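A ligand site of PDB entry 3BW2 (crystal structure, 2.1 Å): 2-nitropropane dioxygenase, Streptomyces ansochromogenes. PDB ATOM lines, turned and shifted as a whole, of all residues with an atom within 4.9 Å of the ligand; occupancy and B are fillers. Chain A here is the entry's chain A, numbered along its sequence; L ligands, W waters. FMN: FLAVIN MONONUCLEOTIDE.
N of Gly 216 is in hydrogen-bond range of O2P of the ligand (2.7 Å). The backbone NH (N) of Thr 238 lies within hydrogen-bond range of an oxygen (O3P) of the ligand (3.0 Å). The side-chain hydroxyl (OG1) of Thr 238 is in hydrogen-bond range of an oxygen (O3P) of the ligand (2.9 Å). The side-chain amide oxygen of Asn 68 is in hydrogen-bond range of a nitrogen (N3) of the ligand. N of Gly 237 sits at hydrogen-bond distance from O1P of the ligand (2.9 Å). NE2 of Gln 235 is in hydrogen-bond range of O2' of the ligand (3.0 Å). O3' of the ligand sits at hydrogen-bond distance from NE2 of Gln 172. An oxygen (O5') of the ligand lies within hydrogen-bond range of the backbone NH of Gly 177, at 3.1 Å. A nitrogen (N5) of the ligand lies within hydrogen-bond range of the backbone NH (N) of Ala 19 (3.3 Å).
The side-chain hydroxyl (OG1) of Thr 238 is in hydrogen-bond range of the backbone NH (N) of Gly 322 (2.8 Å). NE2 of Gln 172 is in hydrogen-bond range of O of His 179, at 3.0 Å. The backbone carbonyl oxygen (O) of Leu 236 lies within hydrogen-bond range of the backbone NH (N) of Ala 16 (2.8 Å). A ring nitrogen (NE2) of His 252 sits at hydrogen-bond distance from the backbone carbonyl oxygen of Trp 320 (2.9 Å). The backbone carbonyl oxygen (O) of Glu 175 is in hydrogen-bond range of the backbone NH (N) of Gln 323.
The backbone carbonyl oxygen (O) of Pro 17 lies close to a nitrogen (N5) of the ligand (3.3 Å). Merely in contact with the ligand: His 129, Phe 70, Met 18, Ala 176, Gly 322, Ala 16, Trp 320, Gly 215, Leu 236, Gly 178, Leu 241 and Glu 175. Within 4 Å of the ligand: Ala 16, Pro 17, Met 18, Ala 19, Asn 68, Phe 70, His 129, Gln 172, Glu 175, Ala 176, Gly 177, Gly 178, Gly 215, Gly 216, Gln 235, Leu 236, Gly 237, Thr 238, Leu 241, Trp 320 and Gly 322.
Water W5 lies within hydrogen-bond range of O1P of the ligand (2.6 Å), O of Gln 235 (2.8 Å), N of Gly 215 (2.9 Å) and N of Ile 217 (3.1 Å). Water W7 lies within hydrogen-bond range of O2 of the ligand (2.8 Å) and NE2 of Gln 235 (3.2 Å). Water W8 lies within hydrogen-bond range of the side-chain amide oxygen (OD1) of Asn 68 (2.9 Å) and an oxygen (O4) of the ligand (2.9 Å). Water W2 lies within hydrogen-bond range of an oxygen (O2P) of the ligand and the backbone carbonyl oxygen of Gly 322. Water W4 lies within hydrogen-bond range of the backbone carbonyl oxygen of Ile 217 (2.7 Å), an oxygen (O1P) of the ligand (3.0 Å) and the backbone NH of Gly 237 (3.4 Å). Water W3 bridges N of His 179 (2.8 Å) and N5 of the ligand (3.3 Å).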
ATOM      1  N   ALA A  16       7.514 -10.222   7.705  1.00  0.00           N
ATOM      2  CA  ALA A  16       7.147  -9.721   9.023  1.00  0.00           C
ATOM      3  C   ALA A  16       7.717  -8.346   9.318  1.00  0.00           C
ATOM      4  O   ALA A  16       8.865  -8.033   8.961  1.00  0.00           O
ATOM      5  CB  ALA A  16       7.603 -10.700  10.091  1.00  0.00           C
ATOM      6  N   PRO A  17       6.912  -7.471   9.941  1.00  0.00           N
ATOM      7  CA  PRO A  17       7.433  -6.147  10.265  1.00  0.00           C
ATOM      8  C   PRO A  17       8.463  -6.405  11.358  1.00  0.00           C
ATOM      9  O   PRO A  17       8.220  -7.209  12.257  1.00  0.00           O
ATOM     10  CB  PRO A  17       6.200  -5.420  10.809  1.00  0.00           C
ATOM     11  CG  PRO A  17       5.412  -6.548  11.440  1.00  0.00           C
ATOM     12  CD  PRO A  17       5.515  -7.622  10.379  1.00  0.00           C
ATOM     13  N   MET A  18       9.621  -5.758  11.276  1.00  0.00           N
ATOM     14  CA  MET A  18      10.662  -5.944  12.274  1.00  0.00           C
ATOM     15  C   MET A  18      11.212  -4.600  12.680  1.00  0.00           C
ATOM     16  O   MET A  18      11.858  -3.908  11.886  1.00  0.00           O
ATOM     17  CB  MET A  18      11.756  -6.863  11.714  1.00  0.00           C
ATOM     18  CG  MET A  18      11.231  -8.256  11.375  1.00  0.00           C
ATOM     19  SD  MET A  18      12.467  -9.434  10.773  1.00  0.00           S
ATOM     20  CE  MET A  18      12.384  -9.132   8.988  1.00  0.00           C
ATOM     21  N   ALA A  19      10.950  -4.213  13.924  1.00  0.00           N
ATOM     22  CA  ALA A  19      11.389  -2.929  14.448  1.00  0.00           C
ATOM     23  C   ALA A  19      12.882  -2.906  14.701  1.00  0.00           C
ATOM     24  O   ALA A  19      13.579  -3.895  14.444  1.00  0.00           O
ATOM     25  CB  ALA A  19      10.638  -2.608  15.734  1.00  0.00           C
ATOM     26  N   VAL A  22      15.269  -2.845  11.282  1.00  0.00           N
ATOM     27  CA  VAL A  22      15.434  -4.015  10.439  1.00  0.00           C
ATOM     28  C   VAL A  22      14.655  -3.918   9.135  1.00  0.00           C
ATOM     29  O   VAL A  22      15.232  -3.959   8.048  1.00  0.00           O
ATOM     30  CB  VAL A  22      15.024  -5.299  11.182  1.00  0.00           C
ATOM     31  CG1 VAL A  22      15.033  -6.492  10.224  1.00  0.00           C
ATOM     32  CG2 VAL A  22      15.977  -5.552  12.344  1.00  0.00           C
ATOM     33  N   ALA A  41       7.758  -1.296  10.004  1.00  0.00           N
ATOM     34  CA  ALA A  41       7.566  -1.430  11.444  1.00  0.00           C
ATOM     35  C   ALA A  41       7.504  -0.038  12.059  1.00  0.00           C
ATOM     36  O   ALA A  41       8.463   0.718  11.966  1.00  0.00           O
ATOM     37  CB  ALA A  41       8.712  -2.215  12.058  1.00  0.00           C
ATOM     38  N   ASN A  68       2.970  -1.972  10.729  1.00  0.00           N
ATOM     39  CA  ASN A  68       2.636  -2.596  12.007  1.00  0.00           C
ATOM     40  C   ASN A  68       2.778  -1.606  13.155  1.00  0.00           C
ATOM     41  O   ASN A  68       3.731  -0.829  13.200  1.00  0.00           O
ATOM     42  CB  ASN A  68       3.546  -3.825  12.210  1.00  0.00           C
ATOM     43  CG  ASN A  68       3.437  -4.418  13.609  1.00  0.00           C
ATOM     44  OD1 ASN A  68       4.179  -4.042  14.512  1.00  0.00           O
ATOM     45  ND2 ASN A  68       2.498  -5.345  13.779  1.00  0.00           N
ATOM     46  N   PHE A  70       2.344  -0.955  17.579  1.00  0.00           N
ATOM     47  CA  PHE A  70       2.255  -1.589  18.905  1.00  0.00           C
ATOM     48  C   PHE A  70       1.098  -0.995  19.692  1.00  0.00           C
ATOM     49  O   PHE A  70       0.851   0.207  19.658  1.00  0.00           O
ATOM     50  CB  PHE A  70       3.545  -1.368  19.700  1.00  0.00           C
ATOM     51  CG  PHE A  70       4.760  -1.998  19.096  1.00  0.00           C
ATOM     52  CD1 PHE A  70       4.660  -2.998  18.141  1.00  0.00           C
ATOM     53  CD2 PHE A  70       6.034  -1.616  19.545  1.00  0.00           C
ATOM     54  CE1 PHE A  70       5.796  -3.621  17.628  1.00  0.00           C
ATOM     55  CE2 PHE A  70       7.182  -2.234  19.037  1.00  0.00           C
ATOM     56  CZ  PHE A  70       7.061  -3.243  18.080  1.00  0.00           C
ATOM     57  N   HIS A 129       0.319  -5.378  17.249  1.00  0.00           N
ATOM     58  CA  HIS A 129       1.040  -6.326  18.101  1.00  0.00           C
ATOM     59  C   HIS A 129       0.850  -5.944  19.560  1.00  0.00           C
ATOM     60  O   HIS A 129       0.662  -4.763  19.879  1.00  0.00           O
ATOM     61  CB  HIS A 129       2.534  -6.322  17.752  1.00  0.00           C
ATOM     62  CG  HIS A 129       3.196  -7.660  17.925  1.00  0.00           C
ATOM     63  ND1 HIS A 129       4.236  -7.867  18.797  1.00  0.00           N
ATOM     64  CD2 HIS A 129       2.971  -8.848  17.316  1.00  0.00           C
ATOM     65  CE1 HIS A 129       4.624  -9.126  18.731  1.00  0.00           C
ATOM     66  NE2 HIS A 129       3.876  -9.746  17.833  1.00  0.00           N
ATOM     67  N   GLN A 172       0.792 -16.668  15.625  1.00  0.00           N
ATOM     68  CA  GLN A 172       2.224 -16.705  15.869  1.00  0.00           C
ATOM     69  C   GLN A 172       2.581 -17.810  16.861  1.00  0.00           C
ATOM     70  O   GLN A 172       2.202 -17.743  18.025  1.00  0.00           O
ATOM     71  CB  GLN A 172       2.704 -15.348  16.394  1.00  0.00           C
ATOM     72  CG  GLN A 172       4.190 -15.290  16.717  1.00  0.00           C
ATOM     73  CD  GLN A 172       4.516 -14.151  17.649  1.00  0.00           C
ATOM     74  OE1 GLN A 172       3.853 -13.968  18.666  1.00  0.00           O
ATOM     75  NE2 GLN A 172       5.546 -13.374  17.310  1.00  0.00           N
ATOM     76  N   GLU A 175       7.742 -20.867  18.137  1.00  0.00           N
ATOM     77  CA  GLU A 175       9.027 -20.854  17.424  1.00  0.00           C
ATOM     78  C   GLU A 175       9.452 -19.479  16.903  1.00  0.00           C
ATOM     79  O   GLU A 175      10.623 -19.273  16.584  1.00  0.00           O
ATOM     80  CB  GLU A 175       8.971 -21.822  16.230  1.00  0.00           C
ATOM     81  CG  GLU A 175       8.528 -23.230  16.570  1.00  0.00           C
ATOM     82  CD  GLU A 175       7.063 -23.463  16.270  1.00  0.00           C
ATOM     83  OE1 GLU A 175       6.222 -22.700  16.791  1.00  0.00           O
ATOM     84  OE2 GLU A 175       6.766 -24.400  15.509  1.00  0.00           O
ATOM     85  N   ALA A 176       8.495 -18.568  16.811  1.00  0.00           N
ATOM     86  CA  ALA A 176       8.725 -17.211  16.307  1.00  0.00           C
ATOM     87  C   ALA A 176       9.889 -16.446  16.932  1.00  0.00           C
ATOM     88  O   ALA A 176      10.183 -16.588  18.120  1.00  0.00           O
ATOM     89  CB  ALA A 176       7.435 -16.390  16.459  1.00  0.00           C
ATOM     90  N   GLY A 177      10.534 -15.625  16.119  1.00  0.00           N
ATOM     91  CA  GLY A 177      11.625 -14.794  16.612  1.00  0.00           C
ATOM     92  C   GLY A 177      11.035 -13.478  17.090  1.00  0.00           C
ATOM     93  O   GLY A 177       9.920 -13.108  16.703  1.00  0.00           O
ATOM     94  N   GLY A 178      11.767 -12.770  17.952  1.00  0.00           N
ATOM     95  CA  GLY A 178      11.257 -11.495  18.445  1.00  0.00           C
ATOM     96  C   GLY A 178      10.189 -11.669  19.511  1.00  0.00           C
ATOM     97  O   GLY A 178      10.076 -12.724  20.132  1.00  0.00           O
ATOM     98  N   HIS A 179       9.388 -10.632  19.705  1.00  0.00           N
ATOM     99  CA  HIS A 179       8.353 -10.663  20.738  1.00  0.00           C
ATOM    100  C   HIS A 179       7.134 -11.530  20.481  1.00  0.00           C
ATOM    101  O   HIS A 179       6.562 -11.521  19.386  1.00  0.00           O
ATOM    102  CB  HIS A 179       7.856  -9.246  21.042  1.00  0.00           C
ATOM    103  CG  HIS A 179       8.782  -8.444  21.901  1.00  0.00           C
ATOM    104  ND1 HIS A 179       9.849  -7.741  21.394  1.00  0.00           N
ATOM    105  CD2 HIS A 179       8.800  -8.244  23.245  1.00  0.00           C
ATOM    106  CE1 HIS A 179      10.491  -7.139  22.376  1.00  0.00           C
ATOM    107  NE2 HIS A 179       9.870  -7.430  23.511  1.00  0.00           N
ATOM    108  N   ALA A 214       2.736 -17.748  11.457  1.00  0.00           N
ATOM    109  CA  ALA A 214       4.056 -17.166  11.713  1.00  0.00           C
ATOM    110  C   ALA A 214       4.847 -17.913  12.775  1.00  0.00           C
ATOM    111  O   ALA A 214       4.313 -18.316  13.821  1.00  0.00           O
ATOM    112  CB  ALA A 214       3.891 -15.704  12.131  1.00  0.00           C
ATOM    113  N   GLY A 215       6.147 -18.096  12.503  1.00  0.00           N
ATOM    114  CA  GLY A 215       7.011 -18.765  13.458  1.00  0.00           C
ATOM    115  C   GLY A 215       7.869 -19.895  12.909  1.00  0.00           C
ATOM    116  O   GLY A 215       7.359 -20.980  12.644  1.00  0.00           O
ATOM    117  N   GLY A 216       9.159 -19.635  12.753  1.00  0.00           N
ATOM    118  CA  GLY A 216      10.081 -20.655  12.265  1.00  0.00           C
ATOM    119  C   GLY A 216      10.035 -21.020  10.785  1.00  0.00           C
ATOM    120  O   GLY A 216      10.716 -21.964  10.373  1.00  0.00           O
ATOM    121  N   ILE A 217       9.269 -20.283   9.987  1.00  0.00           N
ATOM    122  CA  ILE A 217       9.149 -20.578   8.561  1.00  0.00           C
ATOM    123  C   ILE A 217      10.345 -20.032   7.753  1.00  0.00           C
ATOM    124  O   ILE A 217      10.490 -18.825   7.584  1.00  0.00           O
ATOM    125  CB  ILE A 217       7.815 -20.012   8.008  1.00  0.00           C
ATOM    126  CG1 ILE A 217       6.644 -20.602   8.806  1.00  0.00           C
ATOM    127  CG2 ILE A 217       7.662 -20.369   6.531  1.00  0.00           C
ATOM    128  CD1 ILE A 217       5.286 -20.077   8.401  1.00  0.00           C
ATOM    129  N   GLN A 235       3.869 -15.711   7.323  1.00  0.00           N
ATOM    130  CA  GLN A 235       4.595 -14.484   7.654  1.00  0.00           C
ATOM    131  C   GLN A 235       5.969 -14.885   8.155  1.00  0.00           C
ATOM    132  O   GLN A 235       6.098 -15.665   9.105  1.00  0.00           O
ATOM    133  CB  GLN A 235       3.850 -13.687   8.719  1.00  0.00           C
ATOM    134  CG  GLN A 235       4.593 -12.424   9.122  1.00  0.00           C
ATOM    135  CD  GLN A 235       3.751 -11.472   9.945  1.00  0.00           C
ATOM    136  OE1 GLN A 235       2.745 -10.953   9.464  1.00  0.00           O
ATOM    137  NE2 GLN A 235       4.153 -11.246  11.183  1.00  0.00           N
ATOM    138  N   LEU A 236       7.001 -14.342   7.501  1.00  0.00           N
ATOM    139  CA  LEU A 236       8.384 -14.654   7.837  1.00  0.00           C
ATOM    140  C   LEU A 236       9.186 -13.448   8.298  1.00  0.00           C
ATOM    141  O   LEU A 236       9.232 -12.416   7.608  1.00  0.00           O
ATOM    142  CB  LEU A 236       9.097 -15.248   6.617  1.00  0.00           C
ATOM    143  CG  LEU A 236       8.673 -16.587   6.025  1.00  0.00           C
ATOM    144  CD1 LEU A 236       7.212 -16.567   5.590  1.00  0.00           C
ATOM    145  CD2 LEU A 236       9.575 -16.867   4.830  1.00  0.00           C
ATOM    146  N   GLY A 237       9.833 -13.583   9.451  1.00  0.00           N
ATOM    147  CA  GLY A 237      10.657 -12.515   9.969  1.00  0.00           C
ATOM    148  C   GLY A 237      12.131 -12.867   9.785  1.00  0.00           C
ATOM    149  O   GLY A 237      12.811 -12.308   8.924  1.00  0.00           O
ATOM    150  N   THR A 238      12.610 -13.803  10.598  1.00  0.00           N
ATOM    151  CA  THR A 238      14.006 -14.229  10.567  1.00  0.00           C
ATOM    152  C   THR A 238      14.559 -14.525   9.169  1.00  0.00           C
ATOM    153  O   THR A 238      15.695 -14.170   8.849  1.00  0.00           O
ATOM    154  CB  THR A 238      14.218 -15.469  11.477  1.00  0.00           C
ATOM    155  OG1 THR A 238      13.883 -15.126  12.832  1.00  0.00           O
ATOM    156  CG2 THR A 238      15.680 -15.922  11.440  1.00  0.00           C
ATOM    157  N   LEU A 241      15.353 -11.261   7.799  1.00  0.00           N
ATOM    158  CA  LEU A 241      16.302 -10.517   8.631  1.00  0.00           C
ATOM    159  C   LEU A 241      17.703 -10.649   8.053  1.00  0.00           C
ATOM    160  O   LEU A 241      18.526  -9.728   8.141  1.00  0.00           O
ATOM    161  CB  LEU A 241      16.277 -11.083  10.060  1.00  0.00           C
ATOM    162  CG  LEU A 241      17.124 -10.436  11.157  1.00  0.00           C
ATOM    163  CD1 LEU A 241      16.692  -9.008  11.382  1.00  0.00           C
ATOM    164  CD2 LEU A 241      16.951 -11.220  12.449  1.00  0.00           C
ATOM    165  N   HIS A 252      24.335  -9.076  14.097  1.00  0.00           N
ATOM    166  CA  HIS A 252      23.062  -9.755  14.259  1.00  0.00           C
ATOM    167  C   HIS A 252      22.854 -10.730  13.108  1.00  0.00           C
ATOM    168  O   HIS A 252      22.472 -11.883  13.313  1.00  0.00           O
ATOM    169  CB  HIS A 252      21.933  -8.728  14.329  1.00  0.00           C
ATOM    170  CG  HIS A 252      20.610  -9.298  14.742  1.00  0.00           C
ATOM    171  ND1 HIS A 252      19.557  -8.515  15.168  1.00  0.00           N
ATOM    172  CD2 HIS A 252      20.154 -10.575  14.774  1.00  0.00           C
ATOM    173  CE1 HIS A 252      18.515  -9.282  15.433  1.00  0.00           C
ATOM    174  NE2 HIS A 252      18.850 -10.534  15.200  1.00  0.00           N
ATOM    175  N   TRP A 320      17.195 -11.085  18.255  1.00  0.00           N
ATOM    176  CA  TRP A 320      15.900 -11.675  17.916  1.00  0.00           C
ATOM    177  C   TRP A 320      16.053 -12.680  16.767  1.00  0.00           C
ATOM    178  O   TRP A 320      16.636 -12.364  15.726  1.00  0.00           O
ATOM    179  CB  TRP A 320      14.910 -10.588  17.481  1.00  0.00           C
ATOM    180  CG  TRP A 320      14.719  -9.451  18.449  1.00  0.00           C
ATOM    181  CD1 TRP A 320      14.554  -8.130  18.121  1.00  0.00           C
ATOM    182  CD2 TRP A 320      14.624  -9.523  19.873  1.00  0.00           C
ATOM    183  NE1 TRP A 320      14.359  -7.384  19.258  1.00  0.00           N
ATOM    184  CE2 TRP A 320      14.396  -8.215  20.349  1.00  0.00           C
ATOM    185  CE3 TRP A 320      14.716 -10.572  20.812  1.00  0.00           C
ATOM    186  CZ2 TRP A 320      14.247  -7.921  21.717  1.00  0.00           C
ATOM    187  CZ3 TRP A 320      14.574 -10.277  22.167  1.00  0.00           C
ATOM    188  CH2 TRP A 320      14.346  -8.961  22.598  1.00  0.00           C
ATOM    189  N   ALA A 321      15.501 -13.876  16.944  1.00  0.00           N
ATOM    190  CA  ALA A 321      15.600 -14.905  15.916  1.00  0.00           C
ATOM    191  C   ALA A 321      14.661 -16.061  16.226  1.00  0.00           C
ATOM    192  O   ALA A 321      14.509 -16.453  17.388  1.00  0.00           O
ATOM    193  CB  ALA A 321      17.045 -15.405  15.798  1.00  0.00           C
ATOM    194  N   GLY A 322      14.025 -16.610  15.198  1.00  0.00           N
ATOM    195  CA  GLY A 322      13.132 -17.735  15.377  1.00  0.00           C
ATOM    196  C   GLY A 322      13.948 -19.003  15.459  1.00  0.00           C
ATOM    197  O   GLY A 322      15.155 -18.986  15.183  1.00  0.00           O
ATOM    198  N   GLN A 323      13.316 -20.120  15.818  1.00  0.00           N
ATOM    199  CA  GLN A 323      14.032 -21.384  15.944  1.00  0.00           C
ATOM    200  C   GLN A 323      14.627 -21.916  14.641  1.00  0.00           C
ATOM    201  O   GLN A 323      15.426 -22.847  14.672  1.00  0.00           O
ATOM    202  CB  GLN A 323      13.106 -22.430  16.570  1.00  0.00           C
ATOM    203  CG  GLN A 323      12.675 -22.081  17.978  1.00  0.00           C
ATOM    204  CD  GLN A 323      11.936 -23.228  18.651  1.00  0.00           C
ATOM    205  OE1 GLN A 323      11.011 -23.787  18.070  1.00  0.00           O
ATOM    206  NE2 GLN A 323      12.354 -23.577  19.856  1.00  0.00           N
HETATM  207  N1  FMN L   1       6.283  -8.433  15.014  1.00  0.00           N
HETATM  208  C2  FMN L   1       5.522  -7.259  15.076  1.00  0.00           C
HETATM  209  O2  FMN L   1       4.297  -7.314  15.010  1.00  0.00           O
HETATM  210  N3  FMN L   1       6.139  -6.021  15.192  1.00  0.00           N
HETATM  211  C4  FMN L   1       7.508  -5.872  15.251  1.00  0.00           C
HETATM  212  O4  FMN L   1       8.015  -4.747  15.357  1.00  0.00           O
HETATM  213  C4A FMN L   1       8.304  -7.053  15.180  1.00  0.00           C
HETATM  214  N5  FMN L   1       9.692  -6.974  15.217  1.00  0.00           N
HETATM  215  C5A FMN L   1      10.495  -8.122  15.113  1.00  0.00           C
HETATM  216  C6  FMN L   1      11.907  -7.991  15.119  1.00  0.00           C
HETATM  217  C7  FMN L   1      12.784  -9.118  15.018  1.00  0.00           C
HETATM  218  C7M FMN L   1      14.096  -8.813  14.259  1.00  0.00           C
HETATM  219  C8  FMN L   1      12.123 -10.391  14.849  1.00  0.00           C
HETATM  220  C8M FMN L   1      12.730 -11.551  14.068  1.00  0.00           C
HETATM  221  C9  FMN L   1      10.696 -10.548  14.865  1.00  0.00           C
HETATM  222  C9A FMN L   1       9.870  -9.408  14.989  1.00  0.00           C
HETATM  223  N10 FMN L   1       8.454  -9.496  14.985  1.00  0.00           N
HETATM  224  C10 FMN L   1       7.670  -8.331  15.068  1.00  0.00           C
HETATM  225  C1' FMN L   1       7.769 -10.858  15.051  1.00  0.00           C
HETATM  226  C2' FMN L   1       7.320 -11.219  13.611  1.00  0.00           C
HETATM  227  O2' FMN L   1       6.080 -10.577  13.344  1.00  0.00           O
HETATM  228  C3' FMN L   1       7.071 -12.765  13.420  1.00  0.00           C
HETATM  229  O3' FMN L   1       6.097 -13.135  14.391  1.00  0.00           O
HETATM  230  C4' FMN L   1       8.319 -13.638  13.630  1.00  0.00           C
HETATM  231  O4' FMN L   1       9.404 -13.034  12.912  1.00  0.00           O
HETATM  232  C5' FMN L   1       8.071 -15.080  13.110  1.00  0.00           C
HETATM  233  O5' FMN L   1       9.241 -15.936  13.289  1.00  0.00           O
HETATM  234  P   FMN L   1      10.495 -16.126  12.265  1.00  0.00           P
HETATM  235  O1P FMN L   1       9.528 -15.929  11.154  1.00  0.00           O
HETATM  236  O2P FMN L   1      10.627 -17.423  13.043  1.00  0.00           O
HETATM  237  O3P FMN L   1      11.045 -14.871  12.910  1.00  0.00           O
HETATM  238  O   HOH W   1       3.558 -11.838  14.665  1.00  0.00           O
HETATM  239  O   HOH W   2      13.094 -18.989  12.414  1.00  0.00           O
HETATM  240  O   HOH W   3       9.491  -8.210  18.248  1.00  0.00           O
HETATM  241  O   HOH W   4      11.294 -16.528   8.774  1.00  0.00           O
HETATM  242  O   HOH W   5       7.783 -17.584  10.222  1.00  0.00           O
HETATM  243  O   HOH W   6       1.167  -8.422  15.073  1.00  0.00           O
HETATM  244  O   HOH W   7       3.069  -9.109  13.273  1.00  0.00           O
HETATM  245  O   HOH W   8       6.564  -2.478  14.348  1.00  0.00           O
